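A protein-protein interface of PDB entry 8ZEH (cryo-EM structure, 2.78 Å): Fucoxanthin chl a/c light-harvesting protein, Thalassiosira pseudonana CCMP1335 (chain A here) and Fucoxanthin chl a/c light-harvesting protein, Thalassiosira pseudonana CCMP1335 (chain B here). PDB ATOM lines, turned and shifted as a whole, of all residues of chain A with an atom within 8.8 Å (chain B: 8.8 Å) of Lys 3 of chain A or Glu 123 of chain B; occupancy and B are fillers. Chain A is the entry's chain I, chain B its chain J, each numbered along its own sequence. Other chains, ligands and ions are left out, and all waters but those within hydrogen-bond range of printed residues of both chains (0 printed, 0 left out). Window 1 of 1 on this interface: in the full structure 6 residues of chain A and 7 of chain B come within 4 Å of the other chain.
Of the 16 printed residues of chain B, 4 touch a printed residue of chain A. Hydrophobic or aromatic side chains of chain B that line the printed part of chain A: Phe 128. Among the printed residues, 6 pairs touch across the chains. Among the printed residues, Asp or Glu carboxylates within 4 Å of a Lys or Arg side-chain nitrogen of the other chain: Lys 3 of chain A with Glu 123 of chain B (3.5 Å).
NZ of Lys 3 of chain A lies within salt-bridge range of OE1 of Glu 123 of chain B (3.5 Å).
Ala 1 of chain A touches none of the printed residues of chain B. Lys 3 of chain A touches just one residue of chain B: Glu 123 (3.5 Å). Of the printed residues of chain B, Phe 9 of chain A touches Ser 114, Glu 123, Arg 124 and Phe 128. Ile 113 of chain B touches none of the printed residues of chain A. Of the printed residues of chain A, Ser 114 of chain B touches Phe 9 (3.7 Å) and Leu 10 (3.97 Å). Gly 118 of chain B touches none of the printed residues of chain A. Gly 122 of chain B touches none of the printed residues of chain A. Glu 123 of chain B touches just these residues of chain A: Lys 3 and Phe 9. Of the printed residues of chain A, Arg 124 of chain B touches Phe 9. Of the printed residues of chain A, Phe 128 of chain B touches Phe 9. The nearest printed residue of chain A that does not touch Ser 114 of chain B is Glu 11 of chain A (6.8 Å).
O of Ala 1 of chain A is in hydrogen-bond range of NZ of Lys 3 of chain A (3.2 Å). O of Leu 10 of chain A is in hydrogen-bond range of N of Ser 4 of chain A. OH of Tyr 42 of chain B lies within hydrogen-bond range of NH1 of Arg 124 of chain B, 3.0 Å away. OG of Ser 121 of chain B sits close to N of Glu 123 of chain B (3.5 Å). The guanidinium group (NE) of Arg 124 of chain B lies within hydrogen-bond range of the backbone carbonyl oxygen (O) of Phe 128 of chain B, 2.8 Å away. The side-chain carboxylate (OE1) of Glu 125 of chain B sits close to the backbone NH (N) of Phe 128 of chain B, at 3.3 Å.
Among the printed residues, pairs that only touch across the chains: Phe 9 of chain A with Arg 124 of chain B (3.3 Å), Phe 9 of chain A with Ser 114 of chain B (3.7 Å), Phe 9 of chain A with Glu 123 of chain B (3.7 Å), Leu 10 of chain A with Ser 114 of chain B (3.97 Å) and Phe 9 of chain A with Phe 128 of chain B (3.99 Å).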
ATOM      1  N   ALA A   1     -10.664  23.978 -10.782  1.00  0.00           N
ATOM      2  CA  ALA A   1     -11.802  23.129 -11.113  1.00  0.00           C
ATOM      3  C   ALA A   1     -12.811  23.884 -11.959  1.00  0.00           C
ATOM      4  O   ALA A   1     -13.849  24.315 -11.455  1.00  0.00           O
ATOM      5  CB  ALA A   1     -12.460  22.603  -9.847  1.00  0.00           C
ATOM      6  N   GLU A   2     -12.507  24.056 -13.241  1.00  0.00           N
ATOM      7  CA  GLU A   2     -13.417  24.762 -14.133  1.00  0.00           C
ATOM      8  C   GLU A   2     -14.044  25.920 -13.387  1.00  0.00           C
ATOM      9  O   GLU A   2     -15.259  26.087 -13.395  1.00  0.00           O
ATOM     10  CB  GLU A   2     -14.485  23.822 -14.703  1.00  0.00           C
ATOM     11  CG  GLU A   2     -14.843  22.641 -13.818  1.00  0.00           C
ATOM     12  CD  GLU A   2     -15.902  21.749 -14.430  1.00  0.00           C
ATOM     13  OE1 GLU A   2     -16.376  22.063 -15.542  1.00  0.00           O
ATOM     14  OE2 GLU A   2     -16.261  20.733 -13.800  1.00  0.00           O
ATOM     15  N   LYS A   3     -13.213  26.720 -12.733  1.00  0.00           N
ATOM     16  CA  LYS A   3     -13.716  27.861 -11.997  1.00  0.00           C
ATOM     17  C   LYS A   3     -13.649  29.092 -12.875  1.00  0.00           C
ATOM     18  O   LYS A   3     -12.684  29.283 -13.612  1.00  0.00           O
ATOM     19  CB  LYS A   3     -12.898  28.077 -10.732  1.00  0.00           C
ATOM     20  CG  LYS A   3     -13.729  28.448  -9.518  1.00  0.00           C
ATOM     21  CD  LYS A   3     -14.599  27.280  -9.088  1.00  0.00           C
ATOM     22  CE  LYS A   3     -13.754  26.062  -8.759  1.00  0.00           C
ATOM     23  NZ  LYS A   3     -14.593  24.887  -8.401  1.00  0.00           N
ATOM     24  N   SER A   4     -14.672  29.930 -12.804  1.00  0.00           N
ATOM     25  CA  SER A   4     -14.675  31.147 -13.588  1.00  0.00           C
ATOM     26  C   SER A   4     -13.499  32.009 -13.185  1.00  0.00           C
ATOM     27  O   SER A   4     -13.233  32.188 -12.000  1.00  0.00           O
ATOM     28  CB  SER A   4     -15.981  31.906 -13.382  1.00  0.00           C
ATOM     29  OG  SER A   4     -16.235  32.113 -12.006  1.00  0.00           O
ATOM     30  N   ALA A   5     -12.790  32.546 -14.167  1.00  0.00           N
ATOM     31  CA  ALA A   5     -11.658  33.407 -13.874  1.00  0.00           C
ATOM     32  C   ALA A   5     -12.113  34.615 -13.081  1.00  0.00           C
ATOM     33  O   ALA A   5     -11.468  35.007 -12.112  1.00  0.00           O
ATOM     34  CB  ALA A   5     -10.986  33.845 -15.160  1.00  0.00           C
ATOM     35  N   SER A   6     -13.226  35.205 -13.486  1.00  0.00           N
ATOM     36  CA  SER A   6     -13.727  36.388 -12.807  1.00  0.00           C
ATOM     37  C   SER A   6     -14.122  36.060 -11.385  1.00  0.00           C
ATOM     38  O   SER A   6     -13.812  36.810 -10.461  1.00  0.00           O
ATOM     39  CB  SER A   6     -14.926  36.951 -13.562  1.00  0.00           C
ATOM     40  OG  SER A   6     -15.934  35.967 -13.719  1.00  0.00           O
ATOM     41  N   LEU A   7     -14.814  34.942 -11.207  1.00  0.00           N
ATOM     42  CA  LEU A   7     -15.233  34.534  -9.878  1.00  0.00           C
ATOM     43  C   LEU A   7     -14.494  33.270  -9.510  1.00  0.00           C
ATOM     44  O   LEU A   7     -14.910  32.176  -9.877  1.00  0.00           O
ATOM     45  CB  LEU A   7     -16.734  34.297  -9.850  1.00  0.00           C
ATOM     46  CG  LEU A   7     -17.578  35.375 -10.525  1.00  0.00           C
ATOM     47  CD1 LEU A   7     -19.055  35.028 -10.453  1.00  0.00           C
ATOM     48  CD2 LEU A   7     -17.308  36.721  -9.878  1.00  0.00           C
ATOM     49  N   PRO A   8     -13.394  33.408  -8.766  1.00  0.00           N
ATOM     50  CA  PRO A   8     -12.574  32.239  -8.438  1.00  0.00           C
ATOM     51  C   PRO A   8     -13.263  31.293  -7.468  1.00  0.00           C
ATOM     52  O   PRO A   8     -12.781  30.183  -7.262  1.00  0.00           O
ATOM     53  CB  PRO A   8     -11.350  32.865  -7.772  1.00  0.00           C
ATOM     54  CG  PRO A   8     -11.858  34.135  -7.177  1.00  0.00           C
ATOM     55  CD  PRO A   8     -12.891  34.642  -8.139  1.00  0.00           C
ATOM     56  N   PHE A   9     -14.367  31.723  -6.874  1.00  0.00           N
ATOM     57  CA  PHE A   9     -15.064  30.900  -5.897  1.00  0.00           C
ATOM     58  C   PHE A   9     -16.287  30.225  -6.491  1.00  0.00           C
ATOM     59  O   PHE A   9     -17.064  29.607  -5.767  1.00  0.00           O
ATOM     60  CB  PHE A   9     -15.491  31.768  -4.719  1.00  0.00           C
ATOM     61  CG  PHE A   9     -16.219  33.014  -5.128  1.00  0.00           C
ATOM     62  CD1 PHE A   9     -15.518  34.156  -5.478  1.00  0.00           C
ATOM     63  CD2 PHE A   9     -17.601  33.040  -5.173  1.00  0.00           C
ATOM     64  CE1 PHE A   9     -16.183  35.303  -5.861  1.00  0.00           C
ATOM     65  CE2 PHE A   9     -18.273  34.184  -5.554  1.00  0.00           C
ATOM     66  CZ  PHE A   9     -17.563  35.317  -5.899  1.00  0.00           C
ATOM     67  N   LEU A  10     -16.472  30.341  -7.800  1.00  0.00           N
ATOM     68  CA  LEU A  10     -17.663  29.782  -8.428  1.00  0.00           C
ATOM     69  C   LEU A  10     -17.352  29.003  -9.692  1.00  0.00           C
ATOM     70  O   LEU A  10     -16.508  29.410 -10.486  1.00  0.00           O
ATOM     71  CB  LEU A  10     -18.657  30.897  -8.748  1.00  0.00           C
ATOM     72  CG  LEU A  10     -20.003  30.473  -9.334  1.00  0.00           C
ATOM     73  CD1 LEU A  10     -20.699  29.490  -8.405  1.00  0.00           C
ATOM     74  CD2 LEU A  10     -20.878  31.691  -9.582  1.00  0.00           C
ATOM     75  N   GLU A  11     -18.046  27.888  -9.888  1.00  0.00           N
ATOM     76  CA  GLU A  11     -17.838  27.070 -11.076  1.00  0.00           C
ATOM     77  C   GLU A  11     -18.128  27.840 -12.348  1.00  0.00           C
ATOM     78  O   GLU A  11     -19.127  28.550 -12.434  1.00  0.00           O
ATOM     79  CB  GLU A  11     -18.738  25.839 -11.014  1.00  0.00           C
ATOM     80  CG  GLU A  11     -18.964  25.164 -12.354  1.00  0.00           C
ATOM     81  CD  GLU A  11     -17.704  24.533 -12.904  1.00  0.00           C
ATOM     82  OE1 GLU A  11     -17.609  24.376 -14.138  1.00  0.00           O
ATOM     83  OE2 GLU A  11     -16.808  24.203 -12.100  1.00  0.00           O
ATOM     84  N   ALA A  12     -17.265  27.693 -13.344  1.00  0.00           N
ATOM     85  CA  ALA A  12     -17.463  28.387 -14.609  1.00  0.00           C
ATOM     86  C   ALA A  12     -18.774  27.967 -15.245  1.00  0.00           C
ATOM     87  O   ALA A  12     -19.071  26.779 -15.336  1.00  0.00           O
ATOM     88  CB  ALA A  12     -16.306  28.108 -15.550  1.00  0.00           C
ATOM     89  N   PRO A  13     -19.568  28.946 -15.691  1.00  0.00           N
ATOM     90  CA  PRO A  13     -20.873  28.634 -16.277  1.00  0.00           C
ATOM     91  C   PRO A  13     -20.737  27.860 -17.568  1.00  0.00           C
ATOM     92  O   PRO A  13     -19.929  28.228 -18.415  1.00  0.00           O
ATOM     93  CB  PRO A  13     -21.463  30.015 -16.570  1.00  0.00           C
ATOM     94  CG  PRO A  13     -20.715  30.957 -15.688  1.00  0.00           C
ATOM     95  CD  PRO A  13     -19.332  30.393 -15.593  1.00  0.00           C
ATOM     96  N   LEU A  23     -14.914  35.600 -19.918  1.00  0.00           N
ATOM     97  CA  LEU A  23     -14.124  35.446 -18.704  1.00  0.00           C
ATOM     98  C   LEU A  23     -14.881  34.610 -17.696  1.00  0.00           C
ATOM     99  O   LEU A  23     -14.562  34.627 -16.509  1.00  0.00           O
ATOM    100  CB  LEU A  23     -13.777  36.806 -18.102  1.00  0.00           C
ATOM    101  CG  LEU A  23     -13.066  37.835 -18.979  1.00  0.00           C
ATOM    102  CD1 LEU A  23     -12.053  37.152 -19.884  1.00  0.00           C
ATOM    103  CD2 LEU A  23     -14.067  38.631 -19.800  1.00  0.00           C
ATOM    104  N   GLY A  24     -15.893  33.887 -18.157  1.00  0.00           N
ATOM    105  CA  GLY A  24     -16.662  33.034 -17.272  1.00  0.00           C
ATOM    106  C   GLY A  24     -17.577  33.800 -16.341  1.00  0.00           C
ATOM    107  O   GLY A  24     -18.014  33.271 -15.324  1.00  0.00           O
ATOM    108  N   PHE A  25     -17.878  35.044 -16.684  1.00  0.00           N
ATOM    109  CA  PHE A  25     -18.703  35.860 -15.809  1.00  0.00           C
ATOM    110  C   PHE A  25     -20.180  35.780 -16.152  1.00  0.00           C
ATOM    111  O   PHE A  25     -20.693  36.616 -16.891  1.00  0.00           O
ATOM    112  CB  PHE A  25     -18.246  37.316 -15.841  1.00  0.00           C
ATOM    113  CG  PHE A  25     -18.999  38.199 -14.897  1.00  0.00           C
ATOM    114  CD1 PHE A  25     -18.808  38.086 -13.533  1.00  0.00           C
ATOM    115  CD2 PHE A  25     -19.902  39.134 -15.368  1.00  0.00           C
ATOM    116  CE1 PHE A  25     -19.501  38.891 -12.655  1.00  0.00           C
ATOM    117  CE2 PHE A  25     -20.599  39.943 -14.494  1.00  0.00           C
ATOM    118  CZ  PHE A  25     -20.399  39.822 -13.135  1.00  0.00           C
ATOM    119  N   ARG A  29     -26.327  32.864 -14.851  1.00  0.00           N
ATOM    120  CA  ARG A  29     -26.492  31.895 -15.936  1.00  0.00           C
ATOM    121  C   ARG A  29     -27.652  32.206 -16.874  1.00  0.00           C
ATOM    122  O   ARG A  29     -28.509  31.357 -17.101  1.00  0.00           O
ATOM    123  CB  ARG A  29     -26.622  30.479 -15.365  1.00  0.00           C
ATOM    124  CG  ARG A  29     -25.278  29.848 -15.047  1.00  0.00           C
ATOM    125  CD  ARG A  29     -25.427  28.456 -14.459  1.00  0.00           C
ATOM    126  NE  ARG A  29     -24.145  27.759 -14.413  1.00  0.00           N
ATOM    127  CZ  ARG A  29     -23.260  27.884 -13.430  1.00  0.00           C
ATOM    128  NH1 ARG A  29     -23.512  28.683 -12.403  1.00  0.00           N
ATOM    129  NH2 ARG A  29     -22.119  27.210 -13.475  1.00  0.00           N
ATOM    130  N   TYR B  42     -24.002  23.485   6.839  1.00  0.00           N
ATOM    131  CA  TYR B  42     -23.188  24.288   5.945  1.00  0.00           C
ATOM    132  C   TYR B  42     -23.710  25.706   5.954  1.00  0.00           C
ATOM    133  O   TYR B  42     -22.943  26.657   6.089  1.00  0.00           O
ATOM    134  CB  TYR B  42     -23.230  23.732   4.528  1.00  0.00           C
ATOM    135  CG  TYR B  42     -22.196  24.330   3.601  1.00  0.00           C
ATOM    136  CD1 TYR B  42     -21.018  23.654   3.321  1.00  0.00           C
ATOM    137  CD2 TYR B  42     -22.397  25.566   3.005  1.00  0.00           C
ATOM    138  CE1 TYR B  42     -20.068  24.191   2.473  1.00  0.00           C
ATOM    139  CE2 TYR B  42     -21.451  26.113   2.158  1.00  0.00           C
ATOM    140  CZ  TYR B  42     -20.289  25.420   1.897  1.00  0.00           C
ATOM    141  OH  TYR B  42     -19.343  25.957   1.055  1.00  0.00           O
ATOM    142  N   ILE B 113     -25.381  32.357  -4.478  1.00  0.00           N
ATOM    143  CA  ILE B 113     -25.285  31.363  -5.533  1.00  0.00           C
ATOM    144  C   ILE B 113     -24.126  30.430  -5.258  1.00  0.00           C
ATOM    145  O   ILE B 113     -24.271  29.213  -5.339  1.00  0.00           O
ATOM    146  CB  ILE B 113     -25.079  32.022  -6.904  1.00  0.00           C
ATOM    147  CG1 ILE B 113     -26.274  32.909  -7.252  1.00  0.00           C
ATOM    148  CG2 ILE B 113     -24.867  30.962  -7.974  1.00  0.00           C
ATOM    149  CD1 ILE B 113     -26.122  33.644  -8.566  1.00  0.00           C
ATOM    150  N   SER B 114     -22.976  30.993  -4.911  1.00  0.00           N
ATOM    151  CA  SER B 114     -21.804  30.175  -4.649  1.00  0.00           C
ATOM    152  C   SER B 114     -22.049  29.241  -3.478  1.00  0.00           C
ATOM    153  O   SER B 114     -21.707  28.064  -3.537  1.00  0.00           O
ATOM    154  CB  SER B 114     -20.593  31.057  -4.369  1.00  0.00           C
ATOM    155  OG  SER B 114     -20.775  31.817  -3.190  1.00  0.00           O
ATOM    156  N   THR B 115     -22.647  29.758  -2.413  1.00  0.00           N
ATOM    157  CA  THR B 115     -22.916  28.935  -1.246  1.00  0.00           C
ATOM    158  C   THR B 115     -23.838  27.792  -1.611  1.00  0.00           C
ATOM    159  O   THR B 115     -23.559  26.638  -1.296  1.00  0.00           O
ATOM    160  CB  THR B 115     -23.570  29.750  -0.120  1.00  0.00           C
ATOM    161  OG1 THR B 115     -22.710  30.834   0.247  1.00  0.00           O
ATOM    162  CG2 THR B 115     -23.820  28.872   1.096  1.00  0.00           C
ATOM    163  N   THR B 116     -24.944  28.101  -2.273  1.00  0.00           N
ATOM    164  CA  THR B 116     -25.877  27.064  -2.677  1.00  0.00           C
ATOM    165  C   THR B 116     -25.156  25.977  -3.448  1.00  0.00           C
ATOM    166  O   THR B 116     -25.064  24.837  -2.990  1.00  0.00           O
ATOM    167  CB  THR B 116     -26.994  27.635  -3.557  1.00  0.00           C
ATOM    168  OG1 THR B 116     -27.690  28.662  -2.841  1.00  0.00           O
ATOM    169  CG2 THR B 116     -27.974  26.541  -3.944  1.00  0.00           C
ATOM    170  N   THR B 117     -24.627  26.325  -4.614  1.00  0.00           N
ATOM    171  CA  THR B 117     -23.952  25.343  -5.450  1.00  0.00           C
ATOM    172  C   THR B 117     -22.769  24.710  -4.747  1.00  0.00           C
ATOM    173  O   THR B 117     -22.583  23.499  -4.804  1.00  0.00           O
ATOM    174  CB  THR B 117     -23.447  25.985  -6.752  1.00  0.00           C
ATOM    175  OG1 THR B 117     -24.544  26.602  -7.436  1.00  0.00           O
ATOM    176  CG2 THR B 117     -22.818  24.936  -7.653  1.00  0.00           C
ATOM    177  N   GLY B 118     -21.966  25.522  -4.076  1.00  0.00           N
ATOM    178  CA  GLY B 118     -20.786  25.002  -3.416  1.00  0.00           C
ATOM    179  C   GLY B 118     -21.163  23.946  -2.407  1.00  0.00           C
ATOM    180  O   GLY B 118     -20.516  22.909  -2.319  1.00  0.00           O
ATOM    181  N   ARG B 119     -22.218  24.200  -1.648  1.00  0.00           N
ATOM    182  CA  ARG B 119     -22.654  23.249  -0.641  1.00  0.00           C
ATOM    183  C   ARG B 119     -23.022  21.929  -1.286  1.00  0.00           C
ATOM    184  O   ARG B 119     -22.621  20.868  -0.815  1.00  0.00           O
ATOM    185  CB  ARG B 119     -23.846  23.815   0.126  1.00  0.00           C
ATOM    186  CG  ARG B 119     -24.466  22.868   1.136  1.00  0.00           C
ATOM    187  CD  ARG B 119     -25.823  22.390   0.654  1.00  0.00           C
ATOM    188  NE  ARG B 119     -26.635  23.496   0.156  1.00  0.00           N
ATOM    189  CZ  ARG B 119     -27.413  24.256   0.920  1.00  0.00           C
ATOM    190  NH1 ARG B 119     -27.485  24.034   2.225  1.00  0.00           N
ATOM    191  NH2 ARG B 119     -28.116  25.241   0.380  1.00  0.00           N
ATOM    192  N   GLU B 120     -23.782  21.990  -2.370  1.00  0.00           N
ATOM    193  CA  GLU B 120     -24.196  20.773  -3.053  1.00  0.00           C
ATOM    194  C   GLU B 120     -23.009  20.038  -3.646  1.00  0.00           C
ATOM    195  O   GLU B 120     -22.878  18.829  -3.478  1.00  0.00           O
ATOM    196  CB  GLU B 120     -25.190  21.111  -4.160  1.00  0.00           C
ATOM    197  CG  GLU B 120     -26.342  21.987  -3.698  1.00  0.00           C
ATOM    198  CD  GLU B 120     -27.260  22.391  -4.833  1.00  0.00           C
ATOM    199  OE1 GLU B 120     -27.030  21.940  -5.975  1.00  0.00           O
ATOM    200  OE2 GLU B 120     -28.213  23.160  -4.584  1.00  0.00           O
ATOM    201  N   SER B 121     -22.143  20.762  -4.341  1.00  0.00           N
ATOM    202  CA  SER B 121     -20.988  20.143  -4.980  1.00  0.00           C
ATOM    203  C   SER B 121     -19.942  19.693  -3.977  1.00  0.00           C
ATOM    204  O   SER B 121     -19.334  18.637  -4.142  1.00  0.00           O
ATOM    205  CB  SER B 121     -20.360  21.122  -5.970  1.00  0.00           C
ATOM    206  OG  SER B 121     -20.118  22.372  -5.350  1.00  0.00           O
ATOM    207  N   GLY B 122     -19.724  20.488  -2.937  1.00  0.00           N
ATOM    208  CA  GLY B 122     -18.707  20.162  -1.956  1.00  0.00           C
ATOM    209  C   GLY B 122     -17.378  20.776  -2.339  1.00  0.00           C
ATOM    210  O   GLY B 122     -16.378  20.583  -1.649  1.00  0.00           O
ATOM    211  N   GLU B 123     -17.359  21.514  -3.442  1.00  0.00           N
ATOM    212  CA  GLU B 123     -16.127  22.153  -3.893  1.00  0.00           C
ATOM    213  C   GLU B 123     -15.695  23.290  -2.972  1.00  0.00           C
ATOM    214  O   GLU B 123     -14.505  23.477  -2.735  1.00  0.00           O
ATOM    215  CB  GLU B 123     -16.283  22.655  -5.332  1.00  0.00           C
ATOM    216  CG  GLU B 123     -17.388  23.678  -5.537  1.00  0.00           C
ATOM    217  CD  GLU B 123     -16.922  25.106  -5.325  1.00  0.00           C
ATOM    218  OE1 GLU B 123     -15.704  25.319  -5.143  1.00  0.00           O
ATOM    219  OE2 GLU B 123     -17.776  26.016  -5.348  1.00  0.00           O
ATOM    220  N   ARG B 124     -16.652  24.053  -2.455  1.00  0.00           N
ATOM    221  CA  ARG B 124     -16.322  25.176  -1.582  1.00  0.00           C
ATOM    222  C   ARG B 124     -16.415  24.815  -0.113  1.00  0.00           C
ATOM    223  O   ARG B 124     -17.074  23.844   0.252  1.00  0.00           O
ATOM    224  CB  ARG B 124     -17.233  26.371  -1.861  1.00  0.00           C
ATOM    225  CG  ARG B 124     -16.606  27.450  -2.724  1.00  0.00           C
ATOM    226  CD  ARG B 124     -17.367  28.763  -2.611  1.00  0.00           C
ATOM    227  NE  ARG B 124     -17.250  29.354  -1.280  1.00  0.00           N
ATOM    228  CZ  ARG B 124     -18.153  29.216  -0.315  1.00  0.00           C
ATOM    229  NH1 ARG B 124     -19.255  28.509  -0.529  1.00  0.00           N
ATOM    230  NH2 ARG B 124     -17.957  29.791   0.864  1.00  0.00           N
ATOM    231  N   GLU B 125     -15.759  25.598   0.734  1.00  0.00           N
ATOM    232  CA  GLU B 125     -15.820  25.365   2.170  1.00  0.00           C
ATOM    233  C   GLU B 125     -16.461  26.575   2.815  1.00  0.00           C
ATOM    234  O   GLU B 125     -16.240  27.702   2.374  1.00  0.00           O
ATOM    235  CB  GLU B 125     -14.420  25.110   2.726  1.00  0.00           C
ATOM    236  CG  GLU B 125     -14.269  25.308   4.225  1.00  0.00           C
ATOM    237  CD  GLU B 125     -13.825  26.713   4.589  1.00  0.00           C
ATOM    238  OE1 GLU B 125     -13.688  27.554   3.677  1.00  0.00           O
ATOM    239  OE2 GLU B 125     -13.611  26.976   5.791  1.00  0.00           O
ATOM    240  N   PRO B 126     -17.272  26.360   3.856  1.00  0.00           N
ATOM    241  CA  PRO B 126     -17.977  27.508   4.424  1.00  0.00           C
ATOM    242  C   PRO B 126     -17.020  28.633   4.775  1.00  0.00           C
ATOM    243  O   PRO B 126     -16.095  28.416   5.553  1.00  0.00           O
ATOM    244  CB  PRO B 126     -18.596  26.936   5.696  1.00  0.00           C
ATOM    245  CG  PRO B 126     -18.773  25.486   5.408  1.00  0.00           C
ATOM    246  CD  PRO B 126     -17.609  25.101   4.541  1.00  0.00           C
ATOM    247  N   PHE B 128     -15.063  30.374   2.609  1.00  0.00           N
ATOM    248  CA  PHE B 128     -14.046  30.613   1.594  1.00  0.00           C
ATOM    249  C   PHE B 128     -14.536  31.519   0.482  1.00  0.00           C
ATOM    250  O   PHE B 128     -15.622  31.312  -0.057  1.00  0.00           O
ATOM    251  CB  PHE B 128     -13.573  29.298   0.986  1.00  0.00           C
ATOM    252  CG  PHE B 128     -12.924  29.462  -0.355  1.00  0.00           C
ATOM    253  CD1 PHE B 128     -11.624  29.923  -0.455  1.00  0.00           C
ATOM    254  CD2 PHE B 128     -13.618  29.167  -1.514  1.00  0.00           C
ATOM    255  CE1 PHE B 128     -11.024  30.082  -1.688  1.00  0.00           C
ATOM    256  CE2 PHE B 128     -13.026  29.324  -2.751  1.00  0.00           C
ATOM    257  CZ  PHE B 128     -11.726  29.781  -2.838  1.00  0.00           C
